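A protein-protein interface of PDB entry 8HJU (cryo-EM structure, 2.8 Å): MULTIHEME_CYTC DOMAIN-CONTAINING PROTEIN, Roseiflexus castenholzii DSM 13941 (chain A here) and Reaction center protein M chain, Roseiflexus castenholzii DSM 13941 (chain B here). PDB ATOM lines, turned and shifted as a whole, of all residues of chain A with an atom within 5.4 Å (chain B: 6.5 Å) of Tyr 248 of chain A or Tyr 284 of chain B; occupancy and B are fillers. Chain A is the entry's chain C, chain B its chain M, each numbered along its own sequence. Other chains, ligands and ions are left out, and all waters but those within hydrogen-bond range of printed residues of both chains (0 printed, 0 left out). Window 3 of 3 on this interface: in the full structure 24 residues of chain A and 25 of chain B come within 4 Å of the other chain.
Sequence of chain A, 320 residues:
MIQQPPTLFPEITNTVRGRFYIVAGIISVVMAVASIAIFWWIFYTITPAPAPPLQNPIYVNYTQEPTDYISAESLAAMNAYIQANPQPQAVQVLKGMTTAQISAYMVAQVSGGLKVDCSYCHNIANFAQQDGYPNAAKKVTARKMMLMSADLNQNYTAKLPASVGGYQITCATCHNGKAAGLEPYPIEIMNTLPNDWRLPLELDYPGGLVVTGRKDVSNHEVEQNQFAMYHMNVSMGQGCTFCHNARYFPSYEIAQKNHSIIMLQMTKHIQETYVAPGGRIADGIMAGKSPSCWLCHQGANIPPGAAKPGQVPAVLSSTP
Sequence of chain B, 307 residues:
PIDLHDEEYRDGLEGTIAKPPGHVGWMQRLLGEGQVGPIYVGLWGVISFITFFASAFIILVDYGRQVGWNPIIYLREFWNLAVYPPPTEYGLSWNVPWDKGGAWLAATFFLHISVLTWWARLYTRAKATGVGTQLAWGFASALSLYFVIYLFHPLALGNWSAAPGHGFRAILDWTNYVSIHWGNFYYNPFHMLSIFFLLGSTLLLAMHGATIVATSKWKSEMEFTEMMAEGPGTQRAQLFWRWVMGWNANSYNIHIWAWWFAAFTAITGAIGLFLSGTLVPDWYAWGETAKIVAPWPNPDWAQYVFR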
ATOM      1  N   THR A 212     -14.931 -22.643 -19.283  1.00  0.00           N
ATOM      2  CA  THR A 212     -14.883 -23.871 -18.497  1.00  0.00           C
ATOM      3  C   THR A 212     -16.285 -24.349 -18.139  1.00  0.00           C
ATOM      4  O   THR A 212     -17.064 -23.610 -17.531  1.00  0.00           O
ATOM      5  CB  THR A 212     -14.056 -23.652 -17.235  1.00  0.00           C
ATOM      6  OG1 THR A 212     -12.677 -23.513 -17.587  1.00  0.00           O
ATOM      7  CG2 THR A 212     -14.200 -24.822 -16.287  1.00  0.00           C
ATOM      8  N   HIS A 244      -2.765 -17.380 -13.399  1.00  0.00           N
ATOM      9  CA  HIS A 244      -3.633 -18.533 -13.274  1.00  0.00           C
ATOM     10  C   HIS A 244      -3.014 -19.518 -12.306  1.00  0.00           C
ATOM     11  O   HIS A 244      -1.795 -19.675 -12.268  1.00  0.00           O
ATOM     12  CB  HIS A 244      -3.847 -19.215 -14.619  1.00  0.00           C
ATOM     13  CG  HIS A 244      -4.880 -18.564 -15.479  1.00  0.00           C
ATOM     14  ND1 HIS A 244      -6.207 -18.501 -15.129  1.00  0.00           N
ATOM     15  CD2 HIS A 244      -4.780 -17.961 -16.685  1.00  0.00           C
ATOM     16  CE1 HIS A 244      -6.880 -17.883 -16.080  1.00  0.00           C
ATOM     17  NE2 HIS A 244      -6.038 -17.549 -17.040  1.00  0.00           N
ATOM     18  N   ASN A 245      -3.853 -20.158 -11.506  1.00  0.00           N
ATOM     19  CA  ASN A 245      -3.502 -21.427 -10.887  1.00  0.00           C
ATOM     20  C   ASN A 245      -3.979 -22.489 -11.864  1.00  0.00           C
ATOM     21  O   ASN A 245      -5.174 -22.750 -11.976  1.00  0.00           O
ATOM     22  CB  ASN A 245      -4.145 -21.573  -9.515  1.00  0.00           C
ATOM     23  CG  ASN A 245      -3.589 -22.739  -8.739  1.00  0.00           C
ATOM     24  OD1 ASN A 245      -3.193 -23.740  -9.313  1.00  0.00           O
ATOM     25  ND2 ASN A 245      -3.550 -22.610  -7.429  1.00  0.00           N
ATOM     26  N   ALA A 246      -3.043 -23.089 -12.593  1.00  0.00           N
ATOM     27  CA  ALA A 246      -3.404 -23.956 -13.705  1.00  0.00           C
ATOM     28  C   ALA A 246      -4.247 -25.148 -13.292  1.00  0.00           C
ATOM     29  O   ALA A 246      -4.807 -25.812 -14.168  1.00  0.00           O
ATOM     30  CB  ALA A 246      -2.150 -24.443 -14.415  1.00  0.00           C
ATOM     31  N   ARG A 247      -4.382 -25.467 -11.992  1.00  0.00           N
ATOM     32  CA  ARG A 247      -5.292 -26.525 -11.578  1.00  0.00           C
ATOM     33  C   ARG A 247      -6.746 -26.101 -11.731  1.00  0.00           C
ATOM     34  O   ARG A 247      -7.623 -26.954 -11.889  1.00  0.00           O
ATOM     35  CB  ARG A 247      -4.988 -26.955 -10.144  1.00  0.00           C
ATOM     36  CG  ARG A 247      -5.642 -26.144  -9.056  1.00  0.00           C
ATOM     37  CD  ARG A 247      -5.291 -26.716  -7.702  1.00  0.00           C
ATOM     38  NE  ARG A 247      -5.983 -26.035  -6.618  1.00  0.00           N
ATOM     39  CZ  ARG A 247      -6.053 -26.485  -5.373  1.00  0.00           C
ATOM     40  NH1 ARG A 247      -5.474 -27.626  -5.044  1.00  0.00           N
ATOM     41  NH2 ARG A 247      -6.704 -25.792  -4.458  1.00  0.00           N
ATOM     42  N   TYR A 248      -7.020 -24.802 -11.712  1.00  0.00           N
ATOM     43  CA  TYR A 248      -8.357 -24.303 -12.017  1.00  0.00           C
ATOM     44  C   TYR A 248      -8.209 -22.930 -12.648  1.00  0.00           C
ATOM     45  O   TYR A 248      -7.942 -21.950 -11.948  1.00  0.00           O
ATOM     46  CB  TYR A 248      -9.229 -24.240 -10.773  1.00  0.00           C
ATOM     47  CG  TYR A 248     -10.702 -24.182 -11.076  1.00  0.00           C
ATOM     48  CD1 TYR A 248     -11.276 -25.051 -11.984  1.00  0.00           C
ATOM     49  CD2 TYR A 248     -11.521 -23.258 -10.451  1.00  0.00           C
ATOM     50  CE1 TYR A 248     -12.621 -25.006 -12.258  1.00  0.00           C
ATOM     51  CE2 TYR A 248     -12.864 -23.205 -10.719  1.00  0.00           C
ATOM     52  CZ  TYR A 248     -13.409 -24.080 -11.622  1.00  0.00           C
ATOM     53  OH  TYR A 248     -14.752 -24.031 -11.895  1.00  0.00           O
ATOM     54  N   PHE A 249      -8.393 -22.859 -13.951  1.00  0.00           N
ATOM     55  CA  PHE A 249      -8.289 -21.599 -14.673  1.00  0.00           C
ATOM     56  C   PHE A 249      -9.409 -20.620 -14.330  1.00  0.00           C
ATOM     57  O   PHE A 249      -9.156 -19.414 -14.296  1.00  0.00           O
ATOM     58  CB  PHE A 249      -8.250 -21.863 -16.178  1.00  0.00           C
ATOM     59  CG  PHE A 249      -6.962 -22.464 -16.646  1.00  0.00           C
ATOM     60  CD1 PHE A 249      -5.786 -21.755 -16.564  1.00  0.00           C
ATOM     61  CD2 PHE A 249      -6.928 -23.737 -17.163  1.00  0.00           C
ATOM     62  CE1 PHE A 249      -4.605 -22.302 -16.986  1.00  0.00           C
ATOM     63  CE2 PHE A 249      -5.745 -24.286 -17.586  1.00  0.00           C
ATOM     64  CZ  PHE A 249      -4.584 -23.567 -17.495  1.00  0.00           C
ATOM     65  N   PRO A 250     -10.646 -21.056 -14.073  1.00  0.00           N
ATOM     66  CA  PRO A 250     -11.670 -20.089 -13.649  1.00  0.00           C
ATOM     67  C   PRO A 250     -11.358 -19.374 -12.351  1.00  0.00           C
ATOM     68  O   PRO A 250     -12.057 -18.411 -12.023  1.00  0.00           O
ATOM     69  CB  PRO A 250     -12.924 -20.952 -13.506  1.00  0.00           C
ATOM     70  CG  PRO A 250     -12.715 -22.040 -14.420  1.00  0.00           C
ATOM     71  CD  PRO A 250     -11.264 -22.345 -14.418  1.00  0.00           C
ATOM     72  N   SER A 251     -10.348 -19.802 -11.605  1.00  0.00           N
ATOM     73  CA  SER A 251     -10.084 -19.212 -10.302  1.00  0.00           C
ATOM     74  C   SER A 251      -9.333 -17.899 -10.443  1.00  0.00           C
ATOM     75  O   SER A 251      -8.490 -17.739 -11.327  1.00  0.00           O
ATOM     76  CB  SER A 251      -9.285 -20.182  -9.440  1.00  0.00           C
ATOM     77  OG  SER A 251      -8.981 -19.608  -8.188  1.00  0.00           O
ATOM     78  N   TRP B 182     -13.414 -28.776 -19.694  1.00  0.00           N
ATOM     79  CA  TRP B 182     -14.112 -29.510 -18.649  1.00  0.00           C
ATOM     80  C   TRP B 182     -13.410 -29.408 -17.304  1.00  0.00           C
ATOM     81  O   TRP B 182     -13.389 -30.373 -16.539  1.00  0.00           O
ATOM     82  CB  TRP B 182     -14.292 -30.965 -19.064  1.00  0.00           C
ATOM     83  CG  TRP B 182     -14.965 -31.092 -20.388  1.00  0.00           C
ATOM     84  CD1 TRP B 182     -14.506 -31.761 -21.474  1.00  0.00           C
ATOM     85  CD2 TRP B 182     -16.217 -30.513 -20.775  1.00  0.00           C
ATOM     86  NE1 TRP B 182     -15.390 -31.647 -22.511  1.00  0.00           N
ATOM     87  CE2 TRP B 182     -16.451 -30.884 -22.105  1.00  0.00           C
ATOM     88  CE3 TRP B 182     -17.165 -29.726 -20.120  1.00  0.00           C
ATOM     89  CZ2 TRP B 182     -17.590 -30.496 -22.794  1.00  0.00           C
ATOM     90  CZ3 TRP B 182     -18.289 -29.340 -20.804  1.00  0.00           C
ATOM     91  CH2 TRP B 182     -18.494 -29.724 -22.127  1.00  0.00           C
ATOM     92  N   GLY B 183     -12.860 -28.257 -16.995  1.00  0.00           N
ATOM     93  CA  GLY B 183     -12.200 -28.048 -15.708  1.00  0.00           C
ATOM     94  C   GLY B 183     -10.723 -28.435 -15.768  1.00  0.00           C
ATOM     95  O   GLY B 183      -9.927 -27.732 -16.363  1.00  0.00           O
ATOM     96  N   ASN B 184     -10.388 -29.557 -15.151  1.00  0.00           N
ATOM     97  CA  ASN B 184      -9.020 -30.046 -15.121  1.00  0.00           C
ATOM     98  C   ASN B 184      -9.083 -31.561 -15.175  1.00  0.00           C
ATOM     99  O   ASN B 184      -9.580 -32.189 -14.238  1.00  0.00           O
ATOM    100  CB  ASN B 184      -8.309 -29.563 -13.856  1.00  0.00           C
ATOM    101  CG  ASN B 184      -6.842 -29.883 -13.849  1.00  0.00           C
ATOM    102  OD1 ASN B 184      -6.287 -30.339 -14.841  1.00  0.00           O
ATOM    103  ND2 ASN B 184      -6.199 -29.642 -12.721  1.00  0.00           N
ATOM    104  N   PHE B 185      -8.606 -32.149 -16.269  1.00  0.00           N
ATOM    105  CA  PHE B 185      -8.684 -33.597 -16.399  1.00  0.00           C
ATOM    106  C   PHE B 185      -7.849 -34.326 -15.361  1.00  0.00           C
ATOM    107  O   PHE B 185      -7.992 -35.542 -15.226  1.00  0.00           O
ATOM    108  CB  PHE B 185      -8.261 -34.029 -17.801  1.00  0.00           C
ATOM    109  CG  PHE B 185      -9.401 -34.482 -18.659  1.00  0.00           C
ATOM    110  CD1 PHE B 185     -10.503 -33.674 -18.838  1.00  0.00           C
ATOM    111  CD2 PHE B 185      -9.375 -35.714 -19.282  1.00  0.00           C
ATOM    112  CE1 PHE B 185     -11.547 -34.075 -19.620  1.00  0.00           C
ATOM    113  CE2 PHE B 185     -10.424 -36.123 -20.065  1.00  0.00           C
ATOM    114  CZ  PHE B 185     -11.509 -35.300 -20.236  1.00  0.00           C
ATOM    115  N   TYR B 187      -8.317 -34.046 -12.285  1.00  0.00           N
ATOM    116  CA  TYR B 187      -9.301 -34.408 -11.281  1.00  0.00           C
ATOM    117  C   TYR B 187     -10.442 -35.219 -11.861  1.00  0.00           C
ATOM    118  O   TYR B 187     -11.418 -35.492 -11.162  1.00  0.00           O
ATOM    119  CB  TYR B 187      -9.818 -33.153 -10.587  1.00  0.00           C
ATOM    120  CG  TYR B 187      -8.751 -32.525  -9.739  1.00  0.00           C
ATOM    121  CD1 TYR B 187      -8.428 -33.056  -8.507  1.00  0.00           C
ATOM    122  CD2 TYR B 187      -8.033 -31.431 -10.187  1.00  0.00           C
ATOM    123  CE1 TYR B 187      -7.441 -32.506  -7.735  1.00  0.00           C
ATOM    124  CE2 TYR B 187      -7.046 -30.874  -9.418  1.00  0.00           C
ATOM    125  CZ  TYR B 187      -6.756 -31.418  -8.193  1.00  0.00           C
ATOM    126  OH  TYR B 187      -5.775 -30.873  -7.411  1.00  0.00           O
ATOM    127  N   ASN B 188     -10.338 -35.608 -13.116  1.00  0.00           N
ATOM    128  CA  ASN B 188     -11.200 -36.625 -13.682  1.00  0.00           C
ATOM    129  C   ASN B 188     -10.764 -37.966 -13.110  1.00  0.00           C
ATOM    130  O   ASN B 188      -9.653 -38.416 -13.411  1.00  0.00           O
ATOM    131  CB  ASN B 188     -11.096 -36.601 -15.202  1.00  0.00           C
ATOM    132  CG  ASN B 188     -11.995 -37.613 -15.880  1.00  0.00           C
ATOM    133  OD1 ASN B 188     -12.640 -38.428 -15.235  1.00  0.00           O
ATOM    134  ND2 ASN B 188     -12.038 -37.559 -17.197  1.00  0.00           N
ATOM    135  N   ASP B 282     -17.402 -30.005 -14.970  1.00  0.00           N
ATOM    136  CA  ASP B 282     -16.219 -29.420 -14.359  1.00  0.00           C
ATOM    137  C   ASP B 282     -15.624 -30.461 -13.426  1.00  0.00           C
ATOM    138  O   ASP B 282     -16.305 -30.934 -12.513  1.00  0.00           O
ATOM    139  CB  ASP B 282     -16.592 -28.147 -13.601  1.00  0.00           C
ATOM    140  CG  ASP B 282     -15.405 -27.300 -13.261  1.00  0.00           C
ATOM    141  OD1 ASP B 282     -14.330 -27.858 -12.981  1.00  0.00           O
ATOM    142  OD2 ASP B 282     -15.550 -26.065 -13.252  1.00  0.00           O
ATOM    143  N   TRP B 283     -14.365 -30.819 -13.650  1.00  0.00           N
ATOM    144  CA  TRP B 283     -13.760 -31.857 -12.830  1.00  0.00           C
ATOM    145  C   TRP B 283     -13.132 -31.307 -11.562  1.00  0.00           C
ATOM    146  O   TRP B 283     -13.186 -31.961 -10.517  1.00  0.00           O
ATOM    147  CB  TRP B 283     -12.720 -32.634 -13.632  1.00  0.00           C
ATOM    148  CG  TRP B 283     -13.338 -33.576 -14.579  1.00  0.00           C
ATOM    149  CD1 TRP B 283     -13.252 -33.540 -15.928  1.00  0.00           C
ATOM    150  CD2 TRP B 283     -14.170 -34.693 -14.258  1.00  0.00           C
ATOM    151  NE1 TRP B 283     -13.966 -34.564 -16.472  1.00  0.00           N
ATOM    152  CE2 TRP B 283     -14.544 -35.290 -15.467  1.00  0.00           C
ATOM    153  CE3 TRP B 283     -14.631 -35.248 -13.063  1.00  0.00           C
ATOM    154  CZ2 TRP B 283     -15.351 -36.415 -15.524  1.00  0.00           C
ATOM    155  CZ3 TRP B 283     -15.435 -36.358 -13.122  1.00  0.00           C
ATOM    156  CH2 TRP B 283     -15.784 -36.933 -14.342  1.00  0.00           C
ATOM    157  N   TYR B 284     -12.529 -30.124 -11.622  1.00  0.00           N
ATOM    158  CA  TYR B 284     -11.996 -29.532 -10.404  1.00  0.00           C
ATOM    159  C   TYR B 284     -13.116 -29.149  -9.449  1.00  0.00           C
ATOM    160  O   TYR B 284     -13.019 -29.392  -8.243  1.00  0.00           O
ATOM    161  CB  TYR B 284     -11.132 -28.321 -10.736  1.00  0.00           C
ATOM    162  CG  TYR B 284     -10.641 -27.573  -9.524  1.00  0.00           C
ATOM    163  CD1 TYR B 284     -11.395 -26.560  -8.959  1.00  0.00           C
ATOM    164  CD2 TYR B 284      -9.423 -27.874  -8.949  1.00  0.00           C
ATOM    165  CE1 TYR B 284     -10.956 -25.880  -7.865  1.00  0.00           C
ATOM    166  CE2 TYR B 284      -8.978 -27.193  -7.849  1.00  0.00           C
ATOM    167  CZ  TYR B 284      -9.751 -26.197  -7.311  1.00  0.00           C
ATOM    168  OH  TYR B 284      -9.320 -25.501  -6.210  1.00  0.00           O
ATOM    169  N   ALA B 285     -14.184 -28.544  -9.966  1.00  0.00           N
ATOM    170  CA  ALA B 285     -15.322 -28.224  -9.112  1.00  0.00           C
ATOM    171  C   ALA B 285     -15.935 -29.486  -8.526  1.00  0.00           C
ATOM    172  O   ALA B 285     -16.339 -29.504  -7.360  1.00  0.00           O
ATOM    173  CB  ALA B 285     -16.364 -27.432  -9.894  1.00  0.00           C
ATOM    174  N   TRP B 286     -16.009 -30.553  -9.319  1.00  0.00           N
ATOM    175  CA  TRP B 286     -16.469 -31.827  -8.783  1.00  0.00           C
ATOM    176  C   TRP B 286     -15.490 -32.369  -7.752  1.00  0.00           C
ATOM    177  O   TRP B 286     -15.899 -32.957  -6.747  1.00  0.00           O
ATOM    178  CB  TRP B 286     -16.673 -32.831  -9.916  1.00  0.00           C
ATOM    179  CG  TRP B 286     -16.925 -34.215  -9.437  1.00  0.00           C
ATOM    180  CD1 TRP B 286     -18.127 -34.774  -9.155  1.00  0.00           C
ATOM    181  CD2 TRP B 286     -15.944 -35.223  -9.182  1.00  0.00           C
ATOM    182  NE1 TRP B 286     -17.962 -36.066  -8.738  1.00  0.00           N
ATOM    183  CE2 TRP B 286     -16.627 -36.365  -8.747  1.00  0.00           C
ATOM    184  CE3 TRP B 286     -14.553 -35.268  -9.280  1.00  0.00           C
ATOM    185  CZ2 TRP B 286     -15.972 -37.535  -8.407  1.00  0.00           C
ATOM    186  CZ3 TRP B 286     -13.907 -36.428  -8.944  1.00  0.00           C
ATOM    187  CH2 TRP B 286     -14.612 -37.547  -8.513  1.00  0.00           C
ATOM    188  N   GLY B 287     -14.192 -32.174  -7.979  1.00  0.00           N
ATOM    189  CA  GLY B 287     -13.204 -32.658  -7.032  1.00  0.00           C
ATOM    190  C   GLY B 287     -13.277 -31.973  -5.686  1.00  0.00           C
ATOM    191  O   GLY B 287     -12.918 -32.564  -4.668  1.00  0.00           O
ATOM    192  N   GLU B 288     -13.727 -30.720  -5.656  1.00  0.00           N
ATOM    193  CA  GLU B 288     -13.899 -30.037  -4.380  1.00  0.00           C
ATOM    194  C   GLU B 288     -15.084 -30.599  -3.612  1.00  0.00           C
ATOM    195  O   GLU B 288     -15.024 -30.753  -2.389  1.00  0.00           O
ATOM    196  CB  GLU B 288     -14.074 -28.542  -4.603  1.00  0.00           C
ATOM    197  CG  GLU B 288     -12.865 -27.855  -5.178  1.00  0.00           C
ATOM    198  CD  GLU B 288     -13.115 -26.385  -5.422  1.00  0.00           C
ATOM    199  OE1 GLU B 288     -12.398 -25.553  -4.829  1.00  0.00           O
ATOM    200  OE2 GLU B 288     -14.028 -26.063  -6.208  1.00  0.00           O
ATOM    201  N   THR B 289     -16.178 -30.896  -4.311  1.00  0.00           N
ATOM    202  CA  THR B 289     -17.307 -31.556  -3.676  1.00  0.00           C
ATOM    203  C   THR B 289     -17.004 -33.008  -3.347  1.00  0.00           C
ATOM    204  O   THR B 289     -17.678 -33.590  -2.493  1.00  0.00           O
ATOM    205  CB  THR B 289     -18.537 -31.472  -4.573  1.00  0.00           C
ATOM    206  OG1 THR B 289     -18.395 -32.389  -5.663  1.00  0.00           O
ATOM    207  CG2 THR B 289     -18.690 -30.077  -5.121  1.00  0.00           C
ATOM    208  N   VAL B 293      -9.592 -32.698  -3.640  1.00  0.00           N
ATOM    209  CA  VAL B 293      -8.753 -31.560  -3.992  1.00  0.00           C
ATOM    210  C   VAL B 293      -8.078 -31.056  -2.727  1.00  0.00           C
ATOM    211  O   VAL B 293      -8.746 -30.795  -1.722  1.00  0.00           O
ATOM    212  CB  VAL B 293      -9.577 -30.447  -4.657  1.00  0.00           C
ATOM    213  CG1 VAL B 293      -8.788 -29.164  -4.705  1.00  0.00           C
ATOM    214  CG2 VAL B 293      -9.994 -30.856  -6.046  1.00  0.00           C
ATOM    215  N   ALA B 294      -6.764 -30.928  -2.770  1.00  0.00           N
ATOM    216  CA  ALA B 294      -6.034 -30.445  -1.610  1.00  0.00           C
ATOM    217  C   ALA B 294      -6.257 -28.946  -1.441  1.00  0.00           C
ATOM    218  O   ALA B 294      -6.184 -28.201  -2.423  1.00  0.00           O
ATOM    219  CB  ALA B 294      -4.549 -30.741  -1.754  1.00  0.00           C
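ND2 of Asn 184 of chain B is in hydrogen-bond range of O of Arg 247 of chain A (3.2 Å).
The side-chain hydroxyl (OH) of Tyr 248 of chain A lies within hydrogen-bond range of the side-chain carboxylate (OD2) of Asp 282 of chain B, at 2.6 Å.
OH of Tyr 284 of chain B lies within hydrogen-bond range of NH2 of Arg 247 of chain A.
The guanidinium group (NH1) of Arg 247 of chain A is in hydrogen-bond range of the backbone carbonyl oxygen (O) of Ala 294 of chain B.
The side-chain carboxylate (OD1) of Asp 282 of chain B is in hydrogen-bond range of the backbone NH (N) of Tyr 284 of chain B (3.2 Å).
OD1 of Asp 282 of chain B lies within hydrogen-bond range of N of Ala 285 of chain B, 3.1 Å away.
The side-chain hydroxyl of Tyr 284 of chain B is in hydrogen-bond range of the side-chain carboxylate of Glu 288 of chain B (3.4 Å).
O of Gly 287 of chain B is in hydrogen-bond range of N of Val 293 of chain B (3.5 Å).
The backbone NH (N) of Arg 247 of chain A sits close to the side-chain amide oxygen (OD1) of Asn 245 of chain A, at 3.4 Å.
Among the printed residues, merely in contact across the chains: Thr 212 of chain A with Gly 183 of chain B (3.8 Å), Thr 212 of chain A with Asp 282 of chain B (3.5 Å), Arg 247 of chain A with Val 293 of chain B (3.7 Å) and Tyr 248 of chain A with Tyr 284 of chain B (3.3 Å).
Asn 245 of chain A touches none of the printed residues of chain B.
Of chain B, only Asp 282 and Tyr 284 come within 4 Å of Tyr 248 of chain A.
Of the printed residues of chain A, Asn 184 of chain B touches Arg 247.
Of the printed residues of chain A, Val 293 of chain B touches Arg 247.
The nearest printed residue of chain A that does not touch Tyr 284 of chain B is Ser 251 of chain A (6.1 Å).
Printed residues of chain A that touch a printed residue of chain B: Thr 212, Arg 247 and Tyr 248.
Hydrophobic or aromatic side chains of chain A within 4 Å of the printed part of chain B: Tyr 248.
Of the 16 printed residues of chain B, 6 touch a printed residue of chain A.
Along chain B the printed residues that touch a printed residue of chain A span positions 183 to 294.
Among the printed residues, 8 pairs touch across the chains.
Among the printed residues, no Asp or Glu carboxylate lies within 4 Å of a Lys or Arg side-chain nitrogen of the other chain.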
